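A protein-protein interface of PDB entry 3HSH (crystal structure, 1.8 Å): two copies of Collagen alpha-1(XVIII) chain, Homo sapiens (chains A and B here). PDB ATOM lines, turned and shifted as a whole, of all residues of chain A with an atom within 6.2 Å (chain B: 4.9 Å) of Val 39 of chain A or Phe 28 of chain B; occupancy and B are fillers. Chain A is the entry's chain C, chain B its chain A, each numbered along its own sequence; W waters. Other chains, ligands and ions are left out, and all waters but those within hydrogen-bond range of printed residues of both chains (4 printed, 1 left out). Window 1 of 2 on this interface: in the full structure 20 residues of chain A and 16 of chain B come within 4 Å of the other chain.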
ATOM      1  N   SER A   3      33.472  25.923 -19.672  1.00  0.00           N
ATOM      2  CA  SER A   3      32.888  24.602 -19.772  1.00  0.00           C
ATOM      3  C   SER A   3      33.677  23.851 -20.856  1.00  0.00           C
ATOM      4  O   SER A   3      34.914  23.848 -20.841  1.00  0.00           O
ATOM      5  CB  SER A   3      31.396  24.670 -20.097  1.00  0.00           C
ATOM      6  OG  SER A   3      31.176  25.418 -21.273  1.00  0.00           O
ATOM      7  N   PRO A  22      27.210  19.661 -16.412  1.00  0.00           N
ATOM      8  CA  PRO A  22      26.754  20.978 -15.937  1.00  0.00           C
ATOM      9  C   PRO A  22      26.148  21.845 -17.057  1.00  0.00           C
ATOM     10  O   PRO A  22      26.515  21.674 -18.198  1.00  0.00           O
ATOM     11  CB  PRO A  22      28.056  21.644 -15.433  1.00  0.00           C
ATOM     12  CG  PRO A  22      29.049  20.540 -15.312  1.00  0.00           C
ATOM     13  CD  PRO A  22      28.678  19.536 -16.367  1.00  0.00           C
ATOM     14  N   GLU A  23      25.269  22.786 -16.724  1.00  0.00           N
ATOM     15  CA  GLU A  23      24.756  23.733 -17.723  1.00  0.00           C
ATOM     16  C   GLU A  23      25.892  24.408 -18.473  1.00  0.00           C
ATOM     17  O   GLU A  23      26.951  24.671 -17.894  1.00  0.00           O
ATOM     18  CB  GLU A  23      23.906  24.812 -17.046  1.00  0.00           C
ATOM     19  CG  GLU A  23      22.784  24.194 -16.215  1.00  0.00           C
ATOM     20  CD  GLU A  23      21.839  25.197 -15.601  1.00  0.00           C
ATOM     21  OE1 GLU A  23      21.864  26.382 -16.013  1.00  0.00           O
ATOM     22  OE2 GLU A  23      21.048  24.780 -14.717  1.00  0.00           O
ATOM     23  N   GLY A  24      25.669  24.672 -19.764  1.00  0.00           N
ATOM     24  CA  GLY A  24      26.663  25.359 -20.576  1.00  0.00           C
ATOM     25  C   GLY A  24      27.685  24.467 -21.250  1.00  0.00           C
ATOM     26  O   GLY A  24      28.521  24.957 -22.012  1.00  0.00           O
ATOM     27  N   TRP A  25      27.657  23.173 -20.952  1.00  0.00           N
ATOM     28  CA  TRP A  25      28.495  22.220 -21.676  1.00  0.00           C
ATOM     29  C   TRP A  25      27.794  21.775 -22.954  1.00  0.00           C
ATOM     30  O   TRP A  25      26.584  21.575 -22.939  1.00  0.00           O
ATOM     31  CB  TRP A  25      28.776  20.992 -20.805  1.00  0.00           C
ATOM     32  CG  TRP A  25      29.833  21.281 -19.779  1.00  0.00           C
ATOM     33  CD1 TRP A  25      29.694  22.030 -18.644  1.00  0.00           C
ATOM     34  CD2 TRP A  25      31.194  20.836 -19.808  1.00  0.00           C
ATOM     35  NE1 TRP A  25      30.892  22.077 -17.965  1.00  0.00           N
ATOM     36  CE2 TRP A  25      31.825  21.352 -18.655  1.00  0.00           C
ATOM     37  CE3 TRP A  25      31.945  20.056 -20.698  1.00  0.00           C
ATOM     38  CZ2 TRP A  25      33.178  21.126 -18.373  1.00  0.00           C
ATOM     39  CZ3 TRP A  25      33.286  19.827 -20.419  1.00  0.00           C
ATOM     40  CH2 TRP A  25      33.888  20.363 -19.256  1.00  0.00           C
ATOM     41  N   VAL A  37      23.262  21.555 -26.346  1.00  0.00           N
ATOM     42  CA  VAL A  37      23.829  22.285 -25.202  1.00  0.00           C
ATOM     43  C   VAL A  37      23.006  21.997 -23.945  1.00  0.00           C
ATOM     44  O   VAL A  37      21.796  22.017 -23.983  1.00  0.00           O
ATOM     45  CB  VAL A  37      23.994  23.825 -25.464  1.00  0.00           C
ATOM     46  CG1 VAL A  37      22.685  24.475 -25.834  1.00  0.00           C
ATOM     47  CG2 VAL A  37      24.645  24.516 -24.267  1.00  0.00           C
ATOM     48  N   ARG A  38      23.704  21.732 -22.845  1.00  0.00           N
ATOM     49  CA  ARG A  38      23.067  21.455 -21.556  1.00  0.00           C
ATOM     50  C   ARG A  38      22.531  22.767 -20.994  1.00  0.00           C
ATOM     51  O   ARG A  38      23.247  23.768 -20.955  1.00  0.00           O
ATOM     52  CB  ARG A  38      24.105  20.855 -20.611  1.00  0.00           C
ATOM     53  CG  ARG A  38      23.520  20.318 -19.275  1.00  0.00           C
ATOM     54  CD  ARG A  38      22.579  19.104 -19.437  1.00  0.00           C
ATOM     55  NE  ARG A  38      22.514  18.494 -18.108  1.00  0.00           N
ATOM     56  CZ  ARG A  38      21.856  19.010 -17.082  1.00  0.00           C
ATOM     57  NH1 ARG A  38      21.092  20.077 -17.254  1.00  0.00           N
ATOM     58  NH2 ARG A  38      21.913  18.425 -15.890  1.00  0.00           N
ATOM     59  N   VAL A  39      21.258  22.761 -20.608  1.00  0.00           N
ATOM     60  CA  VAL A  39      20.617  23.953 -20.050  1.00  0.00           C
ATOM     61  C   VAL A  39      19.948  23.597 -18.730  1.00  0.00           C
ATOM     62  O   VAL A  39      19.993  22.435 -18.280  1.00  0.00           O
ATOM     63  CB  VAL A  39      19.567  24.557 -21.020  1.00  0.00           C
ATOM     64  CG1 VAL A  39      20.232  24.914 -22.365  1.00  0.00           C
ATOM     65  CG2 VAL A  39      18.398  23.594 -21.256  1.00  0.00           C
ATOM     66  N   GLN A  40      19.335  24.589 -18.081  1.00  0.00           N
ATOM     67  CA  GLN A  40      18.606  24.281 -16.852  1.00  0.00           C
ATOM     68  C   GLN A  40      17.526  23.208 -17.062  1.00  0.00           C
ATOM     69  O   GLN A  40      16.625  23.346 -17.909  1.00  0.00           O
ATOM     70  CB  GLN A  40      17.951  25.546 -16.291  1.00  0.00           C
ATOM     71  CG  GLN A  40      17.148  25.298 -15.015  1.00  0.00           C
ATOM     72  CD  GLN A  40      16.492  26.561 -14.478  1.00  0.00           C
ATOM     73  OE1 GLN A  40      16.899  27.681 -14.809  1.00  0.00           O
ATOM     74  NE2 GLN A  40      15.476  26.382 -13.628  1.00  0.00           N
ATOM     75  N   ASN A  41      17.624  22.133 -16.283  1.00  0.00           N
ATOM     76  CA  ASN A  41      16.632  21.065 -16.345  1.00  0.00           C
ATOM     77  C   ASN A  41      16.441  20.432 -17.716  1.00  0.00           C
ATOM     78  O   ASN A  41      15.345  19.942 -18.045  1.00  0.00           O
ATOM     79  CB  ASN A  41      15.279  21.553 -15.801  1.00  0.00           C
ATOM     80  CG  ASN A  41      14.439  20.425 -15.278  1.00  0.00           C
ATOM     81  OD1 ASN A  41      14.972  19.400 -14.862  1.00  0.00           O
ATOM     82  ND2 ASN A  41      13.113  20.594 -15.309  1.00  0.00           N
ATOM     83  N   GLY A  42      17.499  20.400 -18.528  1.00  0.00           N
ATOM     84  CA  GLY A  42      17.378  19.679 -19.780  1.00  0.00           C
ATOM     85  C   GLY A  42      18.482  20.011 -20.745  1.00  0.00           C
ATOM     86  O   GLY A  42      19.564  20.400 -20.329  1.00  0.00           O
ATOM     87  N   PHE A  43      18.225  19.821 -22.039  1.00  0.00           N
ATOM     88  CA  PHE A  43      19.230  20.164 -23.035  1.00  0.00           C
ATOM     89  C   PHE A  43      18.562  20.589 -24.336  1.00  0.00           C
ATOM     90  O   PHE A  43      17.428  20.206 -24.618  1.00  0.00           O
ATOM     91  CB  PHE A  43      20.255  19.026 -23.264  1.00  0.00           C
ATOM     92  CG  PHE A  43      19.638  17.687 -23.553  1.00  0.00           C
ATOM     93  CD1 PHE A  43      19.239  16.848 -22.524  1.00  0.00           C
ATOM     94  CD2 PHE A  43      19.477  17.250 -24.874  1.00  0.00           C
ATOM     95  CE1 PHE A  43      18.661  15.596 -22.798  1.00  0.00           C
ATOM     96  CE2 PHE A  43      18.904  15.997 -25.153  1.00  0.00           C
ATOM     97  CZ  PHE A  43      18.510  15.173 -24.110  1.00  0.00           C
ATOM     98  N   ARG A  44      19.268  21.411 -25.110  1.00  0.00           N
ATOM     99  CA  ARG A  44      18.688  21.931 -26.332  1.00  0.00           C
ATOM    100  C   ARG A  44      19.508  21.542 -27.531  1.00  0.00           C
ATOM    101  O   ARG A  44      20.708  21.776 -27.565  1.00  0.00           O
ATOM    102  CB  ARG A  44      18.620  23.457 -26.259  1.00  0.00           C
ATOM    103  CG  ARG A  44      17.557  23.971 -25.294  1.00  0.00           C
ATOM    104  CD  ARG A  44      17.606  25.508 -25.312  1.00  0.00           C
ATOM    105  NE  ARG A  44      16.667  26.130 -24.380  1.00  0.00           N
ATOM    106  CZ  ARG A  44      15.408  26.458 -24.679  1.00  0.00           C
ATOM    107  NH1 ARG A  44      14.914  26.192 -25.882  1.00  0.00           N
ATOM    108  NH2 ARG A  44      14.632  27.029 -23.765  1.00  0.00           N
ATOM    109  N   ARG B   6      33.150  29.142 -22.966  1.00  0.00           N
ATOM    110  CA  ARG B   6      33.046  29.946 -21.737  1.00  0.00           C
ATOM    111  C   ARG B   6      31.581  30.108 -21.352  1.00  0.00           C
ATOM    112  O   ARG B   6      30.708  30.181 -22.215  1.00  0.00           O
ATOM    113  CB  ARG B   6      33.610  31.341 -21.981  1.00  0.00           C
ATOM    114  CG  ARG B   6      35.058  31.377 -22.505  1.00  0.00           C
ATOM    115  CD  ARG B   6      36.074  31.281 -21.358  1.00  0.00           C
ATOM    116  NE  ARG B   6      35.878  32.349 -20.376  1.00  0.00           N
ATOM    117  CZ  ARG B   6      36.487  33.534 -20.420  1.00  0.00           C
ATOM    118  NH1 ARG B   6      37.340  33.817 -21.397  1.00  0.00           N
ATOM    119  NH2 ARG B   6      36.241  34.440 -19.484  1.00  0.00           N
ATOM    120  N   LEU B   7      31.280  30.150 -20.057  1.00  0.00           N
ATOM    121  CA  LEU B   7      29.909  30.456 -19.696  1.00  0.00           C
ATOM    122  C   LEU B   7      29.798  31.527 -18.624  1.00  0.00           C
ATOM    123  O   LEU B   7      30.751  31.773 -17.886  1.00  0.00           O
ATOM    124  CB  LEU B   7      29.063  29.203 -19.401  1.00  0.00           C
ATOM    125  CG  LEU B   7      29.290  28.271 -18.213  1.00  0.00           C
ATOM    126  CD1 LEU B   7      30.734  28.291 -17.751  1.00  0.00           C
ATOM    127  CD2 LEU B   7      28.347  28.654 -17.099  1.00  0.00           C
ATOM    128  N   TRP B   8      28.652  32.210 -18.626  1.00  0.00           N
ATOM    129  CA  TRP B   8      28.313  33.225 -17.631  1.00  0.00           C
ATOM    130  C   TRP B   8      26.875  32.980 -17.172  1.00  0.00           C
ATOM    131  O   TRP B   8      26.062  32.376 -17.885  1.00  0.00           O
ATOM    132  CB  TRP B   8      28.415  34.651 -18.202  1.00  0.00           C
ATOM    133  CG  TRP B   8      29.820  35.093 -18.535  1.00  0.00           C
ATOM    134  CD1 TRP B   8      30.618  35.939 -17.811  1.00  0.00           C
ATOM    135  CD2 TRP B   8      30.563  34.749 -19.708  1.00  0.00           C
ATOM    136  NE1 TRP B   8      31.820  36.136 -18.472  1.00  0.00           N
ATOM    137  CE2 TRP B   8      31.810  35.407 -19.630  1.00  0.00           C
ATOM    138  CE3 TRP B   8      30.291  33.954 -20.823  1.00  0.00           C
ATOM    139  CZ2 TRP B   8      32.797  35.279 -20.632  1.00  0.00           C
ATOM    140  CZ3 TRP B   8      31.274  33.823 -21.809  1.00  0.00           C
ATOM    141  CH2 TRP B   8      32.500  34.500 -21.705  1.00  0.00           C
ATOM    142  N   LEU B  26      33.167  29.454 -27.939  1.00  0.00           N
ATOM    143  CA  LEU B  26      31.721  29.499 -27.751  1.00  0.00           C
ATOM    144  C   LEU B  26      31.430  30.139 -26.413  1.00  0.00           C
ATOM    145  O   LEU B  26      32.246  30.093 -25.516  1.00  0.00           O
ATOM    146  CB  LEU B  26      31.078  28.110 -27.822  1.00  0.00           C
ATOM    147  CG  LEU B  26      30.737  27.671 -29.249  1.00  0.00           C
ATOM    148  CD1 LEU B  26      31.990  27.560 -30.070  1.00  0.00           C
ATOM    149  CD2 LEU B  26      29.968  26.339 -29.241  1.00  0.00           C
ATOM    150  N   ILE B  27      30.259  30.754 -26.322  1.00  0.00           N
ATOM    151  CA  ILE B  27      29.851  31.531 -25.162  1.00  0.00           C
ATOM    152  C   ILE B  27      28.437  31.120 -24.813  1.00  0.00           C
ATOM    153  O   ILE B  27      27.547  31.233 -25.657  1.00  0.00           O
ATOM    154  CB  ILE B  27      29.776  33.020 -25.572  1.00  0.00           C
ATOM    155  CG1 ILE B  27      31.179  33.587 -25.796  1.00  0.00           C
ATOM    156  CG2 ILE B  27      28.967  33.844 -24.542  1.00  0.00           C
ATOM    157  CD1 ILE B  27      31.194  34.904 -26.593  1.00  0.00           C
ATOM    158  N   PHE B  28      28.211  30.703 -23.564  1.00  0.00           N
ATOM    159  CA  PHE B  28      26.862  30.311 -23.144  1.00  0.00           C
ATOM    160  C   PHE B  28      26.424  31.216 -22.024  1.00  0.00           C
ATOM    161  O   PHE B  28      27.203  31.516 -21.123  1.00  0.00           O
ATOM    162  CB  PHE B  28      26.833  28.866 -22.631  1.00  0.00           C
ATOM    163  CG  PHE B  28      25.465  28.413 -22.124  1.00  0.00           C
ATOM    164  CD1 PHE B  28      24.447  28.114 -23.013  1.00  0.00           C
ATOM    165  CD2 PHE B  28      25.221  28.269 -20.754  1.00  0.00           C
ATOM    166  CE1 PHE B  28      23.212  27.702 -22.557  1.00  0.00           C
ATOM    167  CE2 PHE B  28      24.001  27.843 -20.299  1.00  0.00           C
ATOM    168  CZ  PHE B  28      22.986  27.570 -21.205  1.00  0.00           C
ATOM    169  N   VAL B  29      25.185  31.678 -22.091  1.00  0.00           N
ATOM    170  CA  VAL B  29      24.606  32.521 -21.046  1.00  0.00           C
ATOM    171  C   VAL B  29      23.460  31.746 -20.388  1.00  0.00           C
ATOM    172  O   VAL B  29      22.477  31.499 -21.045  1.00  0.00           O
ATOM    173  CB  VAL B  29      24.026  33.810 -21.653  1.00  0.00           C
ATOM    174  CG1 VAL B  29      23.548  34.743 -20.558  1.00  0.00           C
ATOM    175  CG2 VAL B  29      25.058  34.509 -22.537  1.00  0.00           C
ATOM    176  N   ALA B  30      23.603  31.396 -19.116  1.00  0.00           N
ATOM    177  CA  ALA B  30      22.677  30.464 -18.471  1.00  0.00           C
ATOM    178  C   ALA B  30      21.262  30.975 -18.321  1.00  0.00           C
ATOM    179  O   ALA B  30      20.310  30.259 -18.620  1.00  0.00           O
ATOM    180  CB  ALA B  30      23.232  30.009 -17.135  1.00  0.00           C
ATOM    181  N   GLU B  33      19.656  31.068 -21.569  1.00  0.00           N
ATOM    182  CA  GLU B  33      19.866  29.799 -22.272  1.00  0.00           C
ATOM    183  C   GLU B  33      20.249  30.047 -23.720  1.00  0.00           C
ATOM    184  O   GLU B  33      19.740  29.383 -24.637  1.00  0.00           O
ATOM    185  CB  GLU B  33      18.664  28.851 -22.165  1.00  0.00           C
ATOM    186  CG  GLU B  33      18.310  28.523 -20.731  1.00  0.00           C
ATOM    187  CD  GLU B  33      17.247  27.435 -20.594  1.00  0.00           C
ATOM    188  OE1 GLU B  33      16.803  26.867 -21.618  1.00  0.00           O
ATOM    189  OE2 GLU B  33      16.852  27.164 -19.438  1.00  0.00           O
ATOM    190  N   GLU B  34      21.162  30.996 -23.914  1.00  0.00           N
ATOM    191  CA  GLU B  34      21.617  31.341 -25.257  1.00  0.00           C
ATOM    192  C   GLU B  34      23.081  30.957 -25.488  1.00  0.00           C
ATOM    193  O   GLU B  34      23.887  30.937 -24.560  1.00  0.00           O
ATOM    194  CB  GLU B  34      21.357  32.822 -25.536  1.00  0.00           C
ATOM    195  CG  GLU B  34      19.850  33.108 -25.686  1.00  0.00           C
ATOM    196  CD  GLU B  34      19.549  34.560 -25.878  1.00  0.00           C
ATOM    197  OE1 GLU B  34      19.926  35.363 -25.009  1.00  0.00           O
ATOM    198  OE2 GLU B  34      18.933  34.906 -26.906  1.00  0.00           O
ATOM    199  N   LEU B  35      23.383  30.582 -26.727  1.00  0.00           N
ATOM    200  CA  LEU B  35      24.704  30.096 -27.094  1.00  0.00           C
ATOM    201  C   LEU B  35      25.170  30.934 -28.290  1.00  0.00           C
ATOM    202  O   LEU B  35      24.385  31.173 -29.220  1.00  0.00           O
ATOM    203  CB  LEU B  35      24.611  28.622 -27.499  1.00  0.00           C
ATOM    204  CG  LEU B  35      25.953  27.981 -27.891  1.00  0.00           C
ATOM    205  CD1 LEU B  35      26.907  27.971 -26.741  1.00  0.00           C
ATOM    206  CD2 LEU B  35      25.719  26.536 -28.451  1.00  0.00           C
ATOM    207  N   ARG B  51      13.823  23.000 -25.463  1.00  0.00           N
ATOM    208  CA  ARG B  51      14.439  22.163 -24.428  1.00  0.00           C
ATOM    209  C   ARG B  51      13.875  20.741 -24.377  1.00  0.00           C
ATOM    210  O   ARG B  51      12.641  20.525 -24.347  1.00  0.00           O
ATOM    211  CB  ARG B  51      14.317  22.803 -23.038  1.00  0.00           C
ATOM    212  CG  ARG B  51      14.677  21.829 -21.890  1.00  0.00           C
ATOM    213  CD  ARG B  51      14.466  22.444 -20.521  1.00  0.00           C
ATOM    214  NE  ARG B  51      13.043  22.659 -20.278  1.00  0.00           N
ATOM    215  CZ  ARG B  51      12.246  21.802 -19.657  1.00  0.00           C
ATOM    216  NH1 ARG B  51      12.723  20.658 -19.178  1.00  0.00           N
ATOM    217  NH2 ARG B  51      10.961  22.094 -19.510  1.00  0.00           N
HETATM  218  O   HOH W   1      15.244  25.491 -18.812  1.00  0.00           O
HETATM  219  O   HOH W   2      17.459  28.786 -25.995  1.00  0.00           O
HETATM  220  O   HOH W   3      14.982  29.626 -22.186  1.00  0.00           O
HETATM  221  O   HOH W   4      20.663  27.290 -18.424  1.00  0.00           O
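No position is printed for both chains.
Of the 12 printed residues of chain B, 3 touch a printed residue of chain A. Hydrophobic or aromatic side chains of chain B within 4 Å of the printed part of chain A: Phe 28. Along chain B the printed residues that touch a printed residue of chain A span positions 28 to 51. Of the 13 printed residues of chain A, 8 touch a printed residue of chain B. Printed residues of chain A that touch a printed residue of chain B: Gly 24, Val 37, Arg 38, Val 39, Gln 40, Asn 41, Phe 43 and Arg 44. Hydrophobic or aromatic side chains of chain A within 4 Å of the printed part of chain B: Val 37 and Val 39. Among the printed residues, Asp or Glu carboxylates within 4 Å of a Lys or Arg side-chain nitrogen of the other chain: Arg 44 of chain A with Glu 33 of chain B (2.9 Å).
Among the printed residues, merely in contact across the chains: Gly 24 of chain A with Phe 28 of chain B, Val 37 of chain A with Phe 28 of chain B, Arg 38 of chain A with Phe 28 of chain B, Val 39 of chain A with Phe 28 of chain B, Val 39 of chain A with Glu 33 of chain B, Gln 40 of chain A with Glu 33 of chain B, Gln 40 of chain A with Arg 51 of chain B and Phe 43 of chain A with Arg 51 of chain B.
The guanidinium group (NE) of Arg 44 of chain A lies within salt-bridge range of the side-chain carboxylate (OE1) of Glu 33 of chain B (2.9 Å). The guanidinium group (NH1) of Arg 51 of chain B sits at hydrogen-bond distance from the backbone carbonyl oxygen (O) of Asn 41 of chain A, 2.9 Å away. N of Arg 51 of chain B lies close to NH1 of Arg 44 of chain A, 3.4 Å away.
Water W1 bridges the side-chain carboxylate (OE2) of Glu 33 of chain B and the backbone carbonyl oxygen (O) of Gln 40 of chain A. Water W2 bridges the backbone carbonyl oxygen of Glu 33 of chain B and the guanidinium group of Arg 44 of chain A. Water W4 lies within hydrogen-bond range of OE1 of Glu 23 of chain A (2.8 Å), O of Ala 30 of chain B (3.0 Å) and N of Gln 40 of chain A (3.0 Å). Water W3 lies within hydrogen-bond range of the guanidinium group (NH2) of Arg 44 of chain A (3.1 Å) and the side-chain carboxylate (OE1) of Glu 33 of chain B (3.4 Å).
The backbone NH (N) of Phe 28 of chain B sits at hydrogen-bond distance from the backbone carbonyl oxygen (O) of Arg 6 of chain B (2.9 Å). The backbone NH (N) of Trp 8 of chain B lies within hydrogen-bond range of the backbone carbonyl oxygen (O) of Phe 28 of chain B. The side-chain hydroxyl (OG) of Ser 3 of chain A is in hydrogen-bond range of the backbone carbonyl oxygen (O) of Gly 24 of chain A, 2.8 Å away. The backbone carbonyl oxygen of Trp 25 of chain A lies within hydrogen-bond range of the backbone NH of Arg 38 of chain A (2.9 Å). The backbone NH of Arg 44 of chain A sits at hydrogen-bond distance from the backbone carbonyl oxygen of Val 37 of chain A. O of Gly 42 of chain A sits close to NH1 of Arg 38 of chain A, at 3.4 Å.
Ser 3 of chain A touches none of the printed residues of chain B. Printed residues of chain B within 4 Å of Gly 24 of chain A: Phe 28 (3.3 Å). Of the printed residues of chain B, Arg 38 of chain A touches Phe 28. Of the printed residues of chain B, Val 39 of chain A touches Phe 28 and Glu 33. Printed residues of chain A within 4 Å of Phe 28 of chain B: Gly 24 (3.3 Å), Val 37 (3.8 Å), Arg 38 (3.8 Å) and Val 39 (3.998 Å). Glu 34 of chain B touches none of the printed residues of chain A. Of the printed residues of chain A, Arg 51 of chain B touches Gln 40 (3.5 Å), Asn 41 (2.9 Å), Phe 43 (3.6 Å) and Arg 44 (3.4 Å). The nearest printed residue of chain B that does not touch Val 37 of chain A is Leu 35 of chain B (4.4 Å).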
